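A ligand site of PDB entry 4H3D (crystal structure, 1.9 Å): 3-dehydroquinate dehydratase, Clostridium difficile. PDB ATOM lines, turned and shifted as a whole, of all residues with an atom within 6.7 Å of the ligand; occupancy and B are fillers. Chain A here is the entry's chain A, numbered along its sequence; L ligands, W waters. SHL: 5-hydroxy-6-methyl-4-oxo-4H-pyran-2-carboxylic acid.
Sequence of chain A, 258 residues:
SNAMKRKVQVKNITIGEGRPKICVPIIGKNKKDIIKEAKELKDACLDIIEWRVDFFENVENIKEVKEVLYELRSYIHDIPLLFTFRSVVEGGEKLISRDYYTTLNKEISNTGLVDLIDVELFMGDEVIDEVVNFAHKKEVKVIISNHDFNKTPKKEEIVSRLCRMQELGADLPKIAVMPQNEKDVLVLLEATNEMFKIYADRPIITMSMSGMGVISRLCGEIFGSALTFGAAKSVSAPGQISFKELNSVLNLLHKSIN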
ATOM      1  N   PRO A  25     -18.830  25.629  -3.235  1.00  0.00           N
ATOM      2  CA  PRO A  25     -17.756  25.850  -4.206  1.00  0.00           C
ATOM      3  C   PRO A  25     -17.529  27.267  -4.694  1.00  0.00           C
ATOM      4  O   PRO A  25     -18.481  28.074  -4.798  1.00  0.00           O
ATOM      5  CB  PRO A  25     -18.173  24.973  -5.402  1.00  0.00           C
ATOM      6  CG  PRO A  25     -19.587  24.748  -5.260  1.00  0.00           C
ATOM      7  CD  PRO A  25     -19.960  24.884  -3.827  1.00  0.00           C
ATOM      8  N   GLU A  50     -14.921  24.789  -1.107  1.00  0.00           N
ATOM      9  CA  GLU A  50     -14.312  23.995  -2.155  1.00  0.00           C
ATOM     10  C   GLU A  50     -13.835  24.902  -3.259  1.00  0.00           C
ATOM     11  O   GLU A  50     -14.629  25.712  -3.782  1.00  0.00           O
ATOM     12  CB  GLU A  50     -15.332  23.009  -2.779  1.00  0.00           C
ATOM     13  CG  GLU A  50     -14.737  22.136  -3.918  1.00  0.00           C
ATOM     14  CD  GLU A  50     -15.773  21.189  -4.602  1.00  0.00           C
ATOM     15  OE1 GLU A  50     -16.948  21.582  -4.753  1.00  0.00           O
ATOM     16  OE2 GLU A  50     -15.388  20.070  -4.999  1.00  0.00           O
ATOM     17  N   ARG A  52     -13.065  24.848  -6.901  1.00  0.00           N
ATOM     18  CA  ARG A  52     -13.146  24.127  -8.168  1.00  0.00           C
ATOM     19  C   ARG A  52     -12.138  24.774  -9.097  1.00  0.00           C
ATOM     20  O   ARG A  52     -12.469  25.685  -9.875  1.00  0.00           O
ATOM     21  CB  ARG A  52     -14.554  24.202  -8.752  1.00  0.00           C
ATOM     22  CG  ARG A  52     -15.525  23.167  -8.130  1.00  0.00           C
ATOM     23  CD  ARG A  52     -15.217  21.748  -8.589  1.00  0.00           C
ATOM     24  NE  ARG A  52     -15.276  21.644 -10.040  1.00  0.00           N
ATOM     25  CZ  ARG A  52     -16.401  21.484 -10.753  1.00  0.00           C
ATOM     26  NH1 ARG A  52     -17.576  21.390 -10.146  1.00  0.00           N
ATOM     27  NH2 ARG A  52     -16.356  21.428 -12.063  1.00  0.00           N
ATOM     28  N   LEU A  82     -11.143  22.629   0.563  1.00  0.00           N
ATOM     29  CA  LEU A  82     -11.105  21.451  -0.296  1.00  0.00           C
ATOM     30  C   LEU A  82     -10.667  21.922  -1.693  1.00  0.00           C
ATOM     31  O   LEU A  82     -11.249  22.843  -2.245  1.00  0.00           O
ATOM     32  CB  LEU A  82     -12.498  20.802  -0.366  1.00  0.00           C
ATOM     33  CG  LEU A  82     -12.785  19.803  -1.495  1.00  0.00           C
ATOM     34  CD1 LEU A  82     -11.765  18.650  -1.556  1.00  0.00           C
ATOM     35  CD2 LEU A  82     -14.211  19.277  -1.386  1.00  0.00           C
ATOM     36  N   THR A  84     -10.257  20.904  -5.575  1.00  0.00           N
ATOM     37  CA  THR A  84     -10.778  19.955  -6.539  1.00  0.00           C
ATOM     38  C   THR A  84     -10.573  20.366  -7.989  1.00  0.00           C
ATOM     39  O   THR A  84     -11.095  21.366  -8.427  1.00  0.00           O
ATOM     40  CB  THR A  84     -12.320  19.805  -6.356  1.00  0.00           C
ATOM     41  OG1 THR A  84     -12.625  19.384  -5.030  1.00  0.00           O
ATOM     42  CG2 THR A  84     -12.928  18.771  -7.410  1.00  0.00           C
ATOM     43  N   ARG A  86     -11.904  19.022 -11.142  1.00  0.00           N
ATOM     44  CA  ARG A  86     -12.860  18.072 -11.700  1.00  0.00           C
ATOM     45  C   ARG A  86     -12.489  17.868 -13.156  1.00  0.00           C
ATOM     46  O   ARG A  86     -12.428  18.839 -13.932  1.00  0.00           O
ATOM     47  CB  ARG A  86     -14.274  18.629 -11.574  1.00  0.00           C
ATOM     48  CG  ARG A  86     -15.359  17.714 -12.088  1.00  0.00           C
ATOM     49  CD  ARG A  86     -15.444  16.390 -11.335  1.00  0.00           C
ATOM     50  NE  ARG A  86     -15.780  16.522  -9.924  1.00  0.00           N
ATOM     51  CZ  ARG A  86     -15.033  16.081  -8.901  1.00  0.00           C
ATOM     52  NH1 ARG A  86     -13.878  15.414  -9.095  1.00  0.00           N
ATOM     53  NH2 ARG A  86     -15.488  16.250  -7.663  1.00  0.00           N
ATOM     54  N   GLU A  90     -15.800  13.828 -15.980  1.00  0.00           N
ATOM     55  CA  GLU A  90     -16.710  13.867 -14.846  1.00  0.00           C
ATOM     56  C   GLU A  90     -17.337  15.257 -14.617  1.00  0.00           C
ATOM     57  O   GLU A  90     -17.691  15.635 -13.506  1.00  0.00           O
ATOM     58  CB  GLU A  90     -16.052  13.265 -13.601  1.00  0.00           C
ATOM     59  CG  GLU A  90     -15.602  11.801 -13.892  1.00  0.00           C
ATOM     60  CD  GLU A  90     -15.519  10.876 -12.669  1.00  0.00           C
ATOM     61  OE1 GLU A  90     -16.023  11.215 -11.574  1.00  0.00           O
ATOM     62  OE2 GLU A  90     -14.949   9.767 -12.836  1.00  0.00           O
ATOM     63  N   ASP A 118      -9.698  16.291  -3.780  1.00  0.00           N
ATOM     64  CA  ASP A 118     -10.653  15.353  -4.346  1.00  0.00           C
ATOM     65  C   ASP A 118     -10.043  14.752  -5.603  1.00  0.00           C
ATOM     66  O   ASP A 118      -9.715  15.480  -6.526  1.00  0.00           O
ATOM     67  CB  ASP A 118     -11.972  16.113  -4.654  1.00  0.00           C
ATOM     68  CG  ASP A 118     -13.020  15.283  -5.458  1.00  0.00           C
ATOM     69  OD1 ASP A 118     -12.646  14.493  -6.370  1.00  0.00           O
ATOM     70  OD2 ASP A 118     -14.241  15.501  -5.199  1.00  0.00           O
ATOM     71  N   SER A 145     -13.724  10.451  -5.548  1.00  0.00           N
ATOM     72  CA  SER A 145     -15.069  10.644  -6.073  1.00  0.00           C
ATOM     73  C   SER A 145     -15.392   9.888  -7.360  1.00  0.00           C
ATOM     74  O   SER A 145     -14.505   9.445  -8.105  1.00  0.00           O
ATOM     75  CB  SER A 145     -15.320  12.140  -6.311  1.00  0.00           C
ATOM     76  OG  SER A 145     -14.347  12.669  -7.216  1.00  0.00           O
ATOM     77  N   ASN A 146     -16.682   9.758  -7.598  1.00  0.00           N
ATOM     78  CA  ASN A 146     -17.179   9.119  -8.797  1.00  0.00           C
ATOM     79  C   ASN A 146     -18.522   9.742  -9.155  1.00  0.00           C
ATOM     80  O   ASN A 146     -19.350  10.048  -8.270  1.00  0.00           O
ATOM     81  CB  ASN A 146     -17.324   7.629  -8.593  1.00  0.00           C
ATOM     82  CG  ASN A 146     -17.905   6.941  -9.782  1.00  0.00           C
ATOM     83  OD1 ASN A 146     -19.044   6.477  -9.741  1.00  0.00           O
ATOM     84  ND2 ASN A 146     -17.160   6.915 -10.884  1.00  0.00           N
ATOM     85  N   HIS A 147     -18.736   9.929 -10.454  1.00  0.00           N
ATOM     86  CA  HIS A 147     -19.925  10.565 -10.956  1.00  0.00           C
ATOM     87  C   HIS A 147     -20.592   9.792 -12.088  1.00  0.00           C
ATOM     88  O   HIS A 147     -19.911   9.206 -12.934  1.00  0.00           O
ATOM     89  CB  HIS A 147     -19.546  11.925 -11.538  1.00  0.00           C
ATOM     90  CG  HIS A 147     -18.918  12.837 -10.541  1.00  0.00           C
ATOM     91  ND1 HIS A 147     -17.604  12.711 -10.139  1.00  0.00           N
ATOM     92  CD2 HIS A 147     -19.405  13.901  -9.887  1.00  0.00           C
ATOM     93  CE1 HIS A 147     -17.330  13.655  -9.254  1.00  0.00           C
ATOM     94  NE2 HIS A 147     -18.410  14.391  -9.080  1.00  0.00           N
ATOM     95  N   PHE A 149     -23.547  10.965 -14.696  1.00  0.00           N
ATOM     96  CA  PHE A 149     -24.461  12.003 -15.109  1.00  0.00           C
ATOM     97  C   PHE A 149     -25.596  11.511 -15.975  1.00  0.00           C
ATOM     98  O   PHE A 149     -26.475  12.275 -16.298  1.00  0.00           O
ATOM     99  CB  PHE A 149     -23.707  13.100 -15.853  1.00  0.00           C
ATOM    100  CG  PHE A 149     -22.881  13.972 -14.965  1.00  0.00           C
ATOM    101  CD1 PHE A 149     -21.593  13.637 -14.669  1.00  0.00           C
ATOM    102  CD2 PHE A 149     -23.419  15.131 -14.435  1.00  0.00           C
ATOM    103  CE1 PHE A 149     -20.825  14.450 -13.828  1.00  0.00           C
ATOM    104  CE2 PHE A 149     -22.660  15.935 -13.599  1.00  0.00           C
ATOM    105  CZ  PHE A 149     -21.374  15.588 -13.294  1.00  0.00           C
ATOM    106  N   LYS A 174     -16.878   9.475  -2.143  1.00  0.00           N
ATOM    107  CA  LYS A 174     -17.912  10.374  -2.633  1.00  0.00           C
ATOM    108  C   LYS A 174     -18.531   9.861  -3.928  1.00  0.00           C
ATOM    109  O   LYS A 174     -17.808   9.527  -4.878  1.00  0.00           O
ATOM    110  CB  LYS A 174     -17.341  11.773  -2.903  1.00  0.00           C
ATOM    111  CG  LYS A 174     -18.393  12.756  -3.489  1.00  0.00           C
ATOM    112  CD  LYS A 174     -17.804  14.120  -3.855  1.00  0.00           C
ATOM    113  CE  LYS A 174     -18.914  15.093  -4.269  1.00  0.00           C
ATOM    114  NZ  LYS A 174     -18.401  16.395  -4.803  1.00  0.00           N
ATOM    115  N   ALA A 176     -21.805  10.763  -6.775  1.00  0.00           N
ATOM    116  CA  ALA A 176     -22.891  11.596  -7.258  1.00  0.00           C
ATOM    117  C   ALA A 176     -23.481  10.914  -8.490  1.00  0.00           C
ATOM    118  O   ALA A 176     -22.765  10.644  -9.463  1.00  0.00           O
ATOM    119  CB  ALA A 176     -22.370  12.983  -7.607  1.00  0.00           C
ATOM    120  N   ILE A 205     -19.927  10.388   1.418  1.00  0.00           N
ATOM    121  CA  ILE A 205     -20.633  11.537   0.840  1.00  0.00           C
ATOM    122  C   ILE A 205     -21.371  11.013  -0.364  1.00  0.00           C
ATOM    123  O   ILE A 205     -20.766  10.384  -1.228  1.00  0.00           O
ATOM    124  CB  ILE A 205     -19.627  12.615   0.351  1.00  0.00           C
ATOM    125  CG1 ILE A 205     -18.631  12.959   1.469  1.00  0.00           C
ATOM    126  CG2 ILE A 205     -20.359  13.862  -0.218  1.00  0.00           C
ATOM    127  CD1 ILE A 205     -17.411  13.788   0.987  1.00  0.00           C
ATOM    128  N   MET A 207     -24.939  11.813  -3.151  1.00  0.00           N
ATOM    129  CA  MET A 207     -25.989  12.661  -3.580  1.00  0.00           C
ATOM    130  C   MET A 207     -26.628  12.167  -4.878  1.00  0.00           C
ATOM    131  O   MET A 207     -25.988  11.440  -5.675  1.00  0.00           O
ATOM    132  CB  MET A 207     -25.477  14.102  -3.754  1.00  0.00           C
ATOM    133  CG  MET A 207     -24.571  14.282  -4.936  1.00  0.00           C
ATOM    134  SD  MET A 207     -23.882  15.956  -4.950  1.00  0.00           S
ATOM    135  CE  MET A 207     -22.671  15.781  -3.649  1.00  0.00           C
ATOM    136  N   MET A 209     -28.323  13.803  -8.072  1.00  0.00           N
ATOM    137  CA  MET A 209     -28.329  15.094  -8.718  1.00  0.00           C
ATOM    138  C   MET A 209     -29.694  15.475  -9.301  1.00  0.00           C
ATOM    139  O   MET A 209     -30.646  14.691  -9.263  1.00  0.00           O
ATOM    140  CB  MET A 209     -27.238  15.130  -9.799  1.00  0.00           C
ATOM    141  CG  MET A 209     -25.807  15.038  -9.223  1.00  0.00           C
ATOM    142  SD  MET A 209     -24.524  15.104 -10.478  1.00  0.00           S
ATOM    143  CE  MET A 209     -24.750  13.559 -11.314  1.00  0.00           C
ATOM    144  N   SER A 210     -29.760  16.720  -9.803  1.00  0.00           N
ATOM    145  CA  SER A 210     -30.949  17.317 -10.449  1.00  0.00           C
ATOM    146  C   SER A 210     -32.015  17.706  -9.426  1.00  0.00           C
ATOM    147  O   SER A 210     -31.898  17.399  -8.248  1.00  0.00           O
ATOM    148  CB  SER A 210     -31.556  16.387 -11.517  1.00  0.00           C
ATOM    149  OG  SER A 210     -32.381  15.400 -10.943  1.00  0.00           O
ATOM    150  N   ARG A 217     -29.798  15.957  -0.541  1.00  0.00           N
ATOM    151  CA  ARG A 217     -28.875  16.935   0.022  1.00  0.00           C
ATOM    152  C   ARG A 217     -29.317  17.377   1.404  1.00  0.00           C
ATOM    153  O   ARG A 217     -28.572  18.046   2.119  1.00  0.00           O
ATOM    154  CB  ARG A 217     -28.793  18.176  -0.860  1.00  0.00           C
ATOM    155  CG  ARG A 217     -28.408  17.907  -2.281  1.00  0.00           C
ATOM    156  CD  ARG A 217     -28.448  19.160  -3.100  1.00  0.00           C
ATOM    157  NE  ARG A 217     -28.139  18.894  -4.510  1.00  0.00           N
ATOM    158  CZ  ARG A 217     -26.932  18.971  -5.048  1.00  0.00           C
ATOM    159  NH1 ARG A 217     -25.883  19.313  -4.305  1.00  0.00           N
ATOM    160  NH2 ARG A 217     -26.773  18.716  -6.329  1.00  0.00           N
ATOM    161  N   THR A 228     -22.725  17.835   2.594  1.00  0.00           N
ATOM    162  CA  THR A 228     -23.715  18.229   1.632  1.00  0.00           C
ATOM    163  C   THR A 228     -23.242  19.525   0.981  1.00  0.00           C
ATOM    164  O   THR A 228     -22.629  20.366   1.627  1.00  0.00           O
ATOM    165  CB  THR A 228     -25.131  18.388   2.258  1.00  0.00           C
ATOM    166  OG1 THR A 228     -26.080  18.693   1.230  1.00  0.00           O
ATOM    167  CG2 THR A 228     -25.142  19.496   3.324  1.00  0.00           C
ATOM    168  N   PHE A 229     -23.512  19.654  -0.300  1.00  0.00           N
ATOM    169  CA  PHE A 229     -23.063  20.784  -1.069  1.00  0.00           C
ATOM    170  C   PHE A 229     -24.174  21.786  -1.405  1.00  0.00           C
ATOM    171  O   PHE A 229     -25.216  21.410  -1.984  1.00  0.00           O
ATOM    172  CB  PHE A 229     -22.389  20.281  -2.345  1.00  0.00           C
ATOM    173  CG  PHE A 229     -21.075  19.601  -2.099  1.00  0.00           C
ATOM    174  CD1 PHE A 229     -21.025  18.311  -1.576  1.00  0.00           C
ATOM    175  CD2 PHE A 229     -19.877  20.241  -2.409  1.00  0.00           C
ATOM    176  CE1 PHE A 229     -19.802  17.688  -1.346  1.00  0.00           C
ATOM    177  CE2 PHE A 229     -18.660  19.599  -2.193  1.00  0.00           C
ATOM    178  CZ  PHE A 229     -18.634  18.315  -1.656  1.00  0.00           C
ATOM    179  N   GLY A 230     -23.937  23.039  -1.056  1.00  0.00           N
ATOM    180  CA  GLY A 230     -24.871  24.132  -1.370  1.00  0.00           C
ATOM    181  C   GLY A 230     -24.271  25.032  -2.431  1.00  0.00           C
ATOM    182  O   GLY A 230     -23.075  24.975  -2.691  1.00  0.00           O
ATOM    183  N   GLY A 239     -31.787  21.895  -9.197  1.00  0.00           N
ATOM    184  CA  GLY A 239     -30.960  20.826  -8.687  1.00  0.00           C
ATOM    185  C   GLY A 239     -29.896  21.292  -7.677  1.00  0.00           C
ATOM    186  O   GLY A 239     -29.083  20.473  -7.224  1.00  0.00           O
ATOM    187  N   GLN A 240     -29.883  22.592  -7.350  1.00  0.00           N
ATOM    188  CA  GLN A 240     -28.940  23.164  -6.366  1.00  0.00           C
ATOM    189  C   GLN A 240     -29.736  23.954  -5.317  1.00  0.00           C
ATOM    190  O   GLN A 240     -30.827  24.453  -5.595  1.00  0.00           O
ATOM    191  CB  GLN A 240     -27.932  24.107  -7.034  1.00  0.00           C
ATOM    192  CG  GLN A 240     -26.983  23.470  -8.089  1.00  0.00           C
ATOM    193  CD  GLN A 240     -25.914  22.518  -7.494  1.00  0.00           C
ATOM    194  OE1 GLN A 240     -25.651  22.509  -6.278  1.00  0.00           O
ATOM    195  NE2 GLN A 240     -25.291  21.720  -8.371  1.00  0.00           N
HETATM  196  OAD SHL L   1     -24.383  19.010  -7.484  1.00  0.00           O
HETATM  197  CAH SHL L   1     -23.414  19.002  -6.674  1.00  0.00           C
HETATM  198  OAA SHL L   1     -23.438  19.675  -5.622  1.00  0.00           O
HETATM  199  CAK SHL L   1     -22.223  18.237  -6.948  1.00  0.00           C
HETATM  200  OAG SHL L   1     -21.249  18.193  -5.891  1.00  0.00           O
HETATM  201  CAF SHL L   1     -20.036  17.553  -6.107  1.00  0.00           C
HETATM  202  CAL SHL L   1     -19.122  17.614  -5.111  1.00  0.00           C
HETATM  203  CAJ SHL L   1     -19.826  16.997  -7.319  1.00  0.00           C
HETATM  204  OAC SHL L   1     -18.655  16.381  -7.574  1.00  0.00           O
HETATM  205  CAI SHL L   1     -20.791  17.030  -8.292  1.00  0.00           C
HETATM  206  CAE SHL L   1     -21.984  17.604  -8.102  1.00  0.00           C
HETATM  207  OAB SHL L   1     -20.547  16.441  -9.469  1.00  0.00           O
HETATM  208  O   HOH W   1     -15.950  17.235  -3.927  1.00  0.00           O
HETATM  209  O   HOH W   2     -21.237  21.311  -5.658  1.00  0.00           O
HETATM  210  O   HOH W   3     -18.837  17.271 -11.560  1.00  0.00           O
HETATM  211  O   HOH W   4     -25.265  19.112  -9.914  1.00  0.00           O
HETATM  212  O   HOH W   5     -16.889  18.762  -6.838  1.00  0.00           O
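The side-chain amino group of Lys 174 is bonded to a carbon (CAL) of the ligand, at 1.4 Å. An oxygen (OAC) of the ligand sits at hydrogen-bond distance from a ring nitrogen (NE2) of His 147, 2.5 Å away. The guanidinium group (NH2) of Arg 86 is in hydrogen-bond range of an oxygen (OAC) of the ligand, at 3.2 Å. The guanidinium group (NH2) of Arg 217 is in salt-bridge range of an oxygen (OAD) of the ligand. An oxygen (OAD) of the ligand lies within hydrogen-bond range of the side-chain amide nitrogen (NE2) of Gln 240, at 3.0 Å.
The side-chain sulfur of Met 207 lies close to an oxygen (OAG) of the ligand. Residues that only touch the ligand: Phe 229. Hydrophobic or aromatic side chains within 4 Å of the ligand: His 147, Met 207 and Phe 229.
NE of Arg 86 sits close to NE2 of His 147, at 3.5 Å. O of Gly 239 lies within hydrogen-bond range of NH2 of Arg 217. OG1 of Thr 228 is in hydrogen-bond range of O of Arg 217 (2.7 Å). The side-chain carboxylate (OD2) of Asp 118 lies within salt-bridge range of the guanidinium group (NH2) of Arg 86 (2.9 Å). N of Asn 146 lies within hydrogen-bond range of O of Lys 174 (3.0 Å). NH1 of Arg 217 is in hydrogen-bond range of O of Phe 229. NH1 of Arg 86 lies within hydrogen-bond range of OG of Ser 145 (3.4 Å). ND1 of His 147 sits at hydrogen-bond distance from OE1 of Glu 90 (2.6 Å).
Water W4 bridges an oxygen (OAD) of the ligand and the side-chain amide nitrogen (NE2) of Gln 240. Water W3 bridges O of Glu 90 (2.8 Å) and OAB of the ligand (2.8 Å). Water W5 lies within hydrogen-bond range of the side-chain carboxylate of Glu 50 (2.7 Å), the guanidinium group of Arg 86 (3.0 Å), an oxygen (OAC) of the ligand (3.1 Å) and the side-chain amino group of Lys 174 (3.5 Å). Water W1 lies within hydrogen-bond range of NZ of Lys 174 (2.7 Å), OD2 of Asp 118 (2.7 Å) and OE2 of Glu 50 (3.1 Å).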
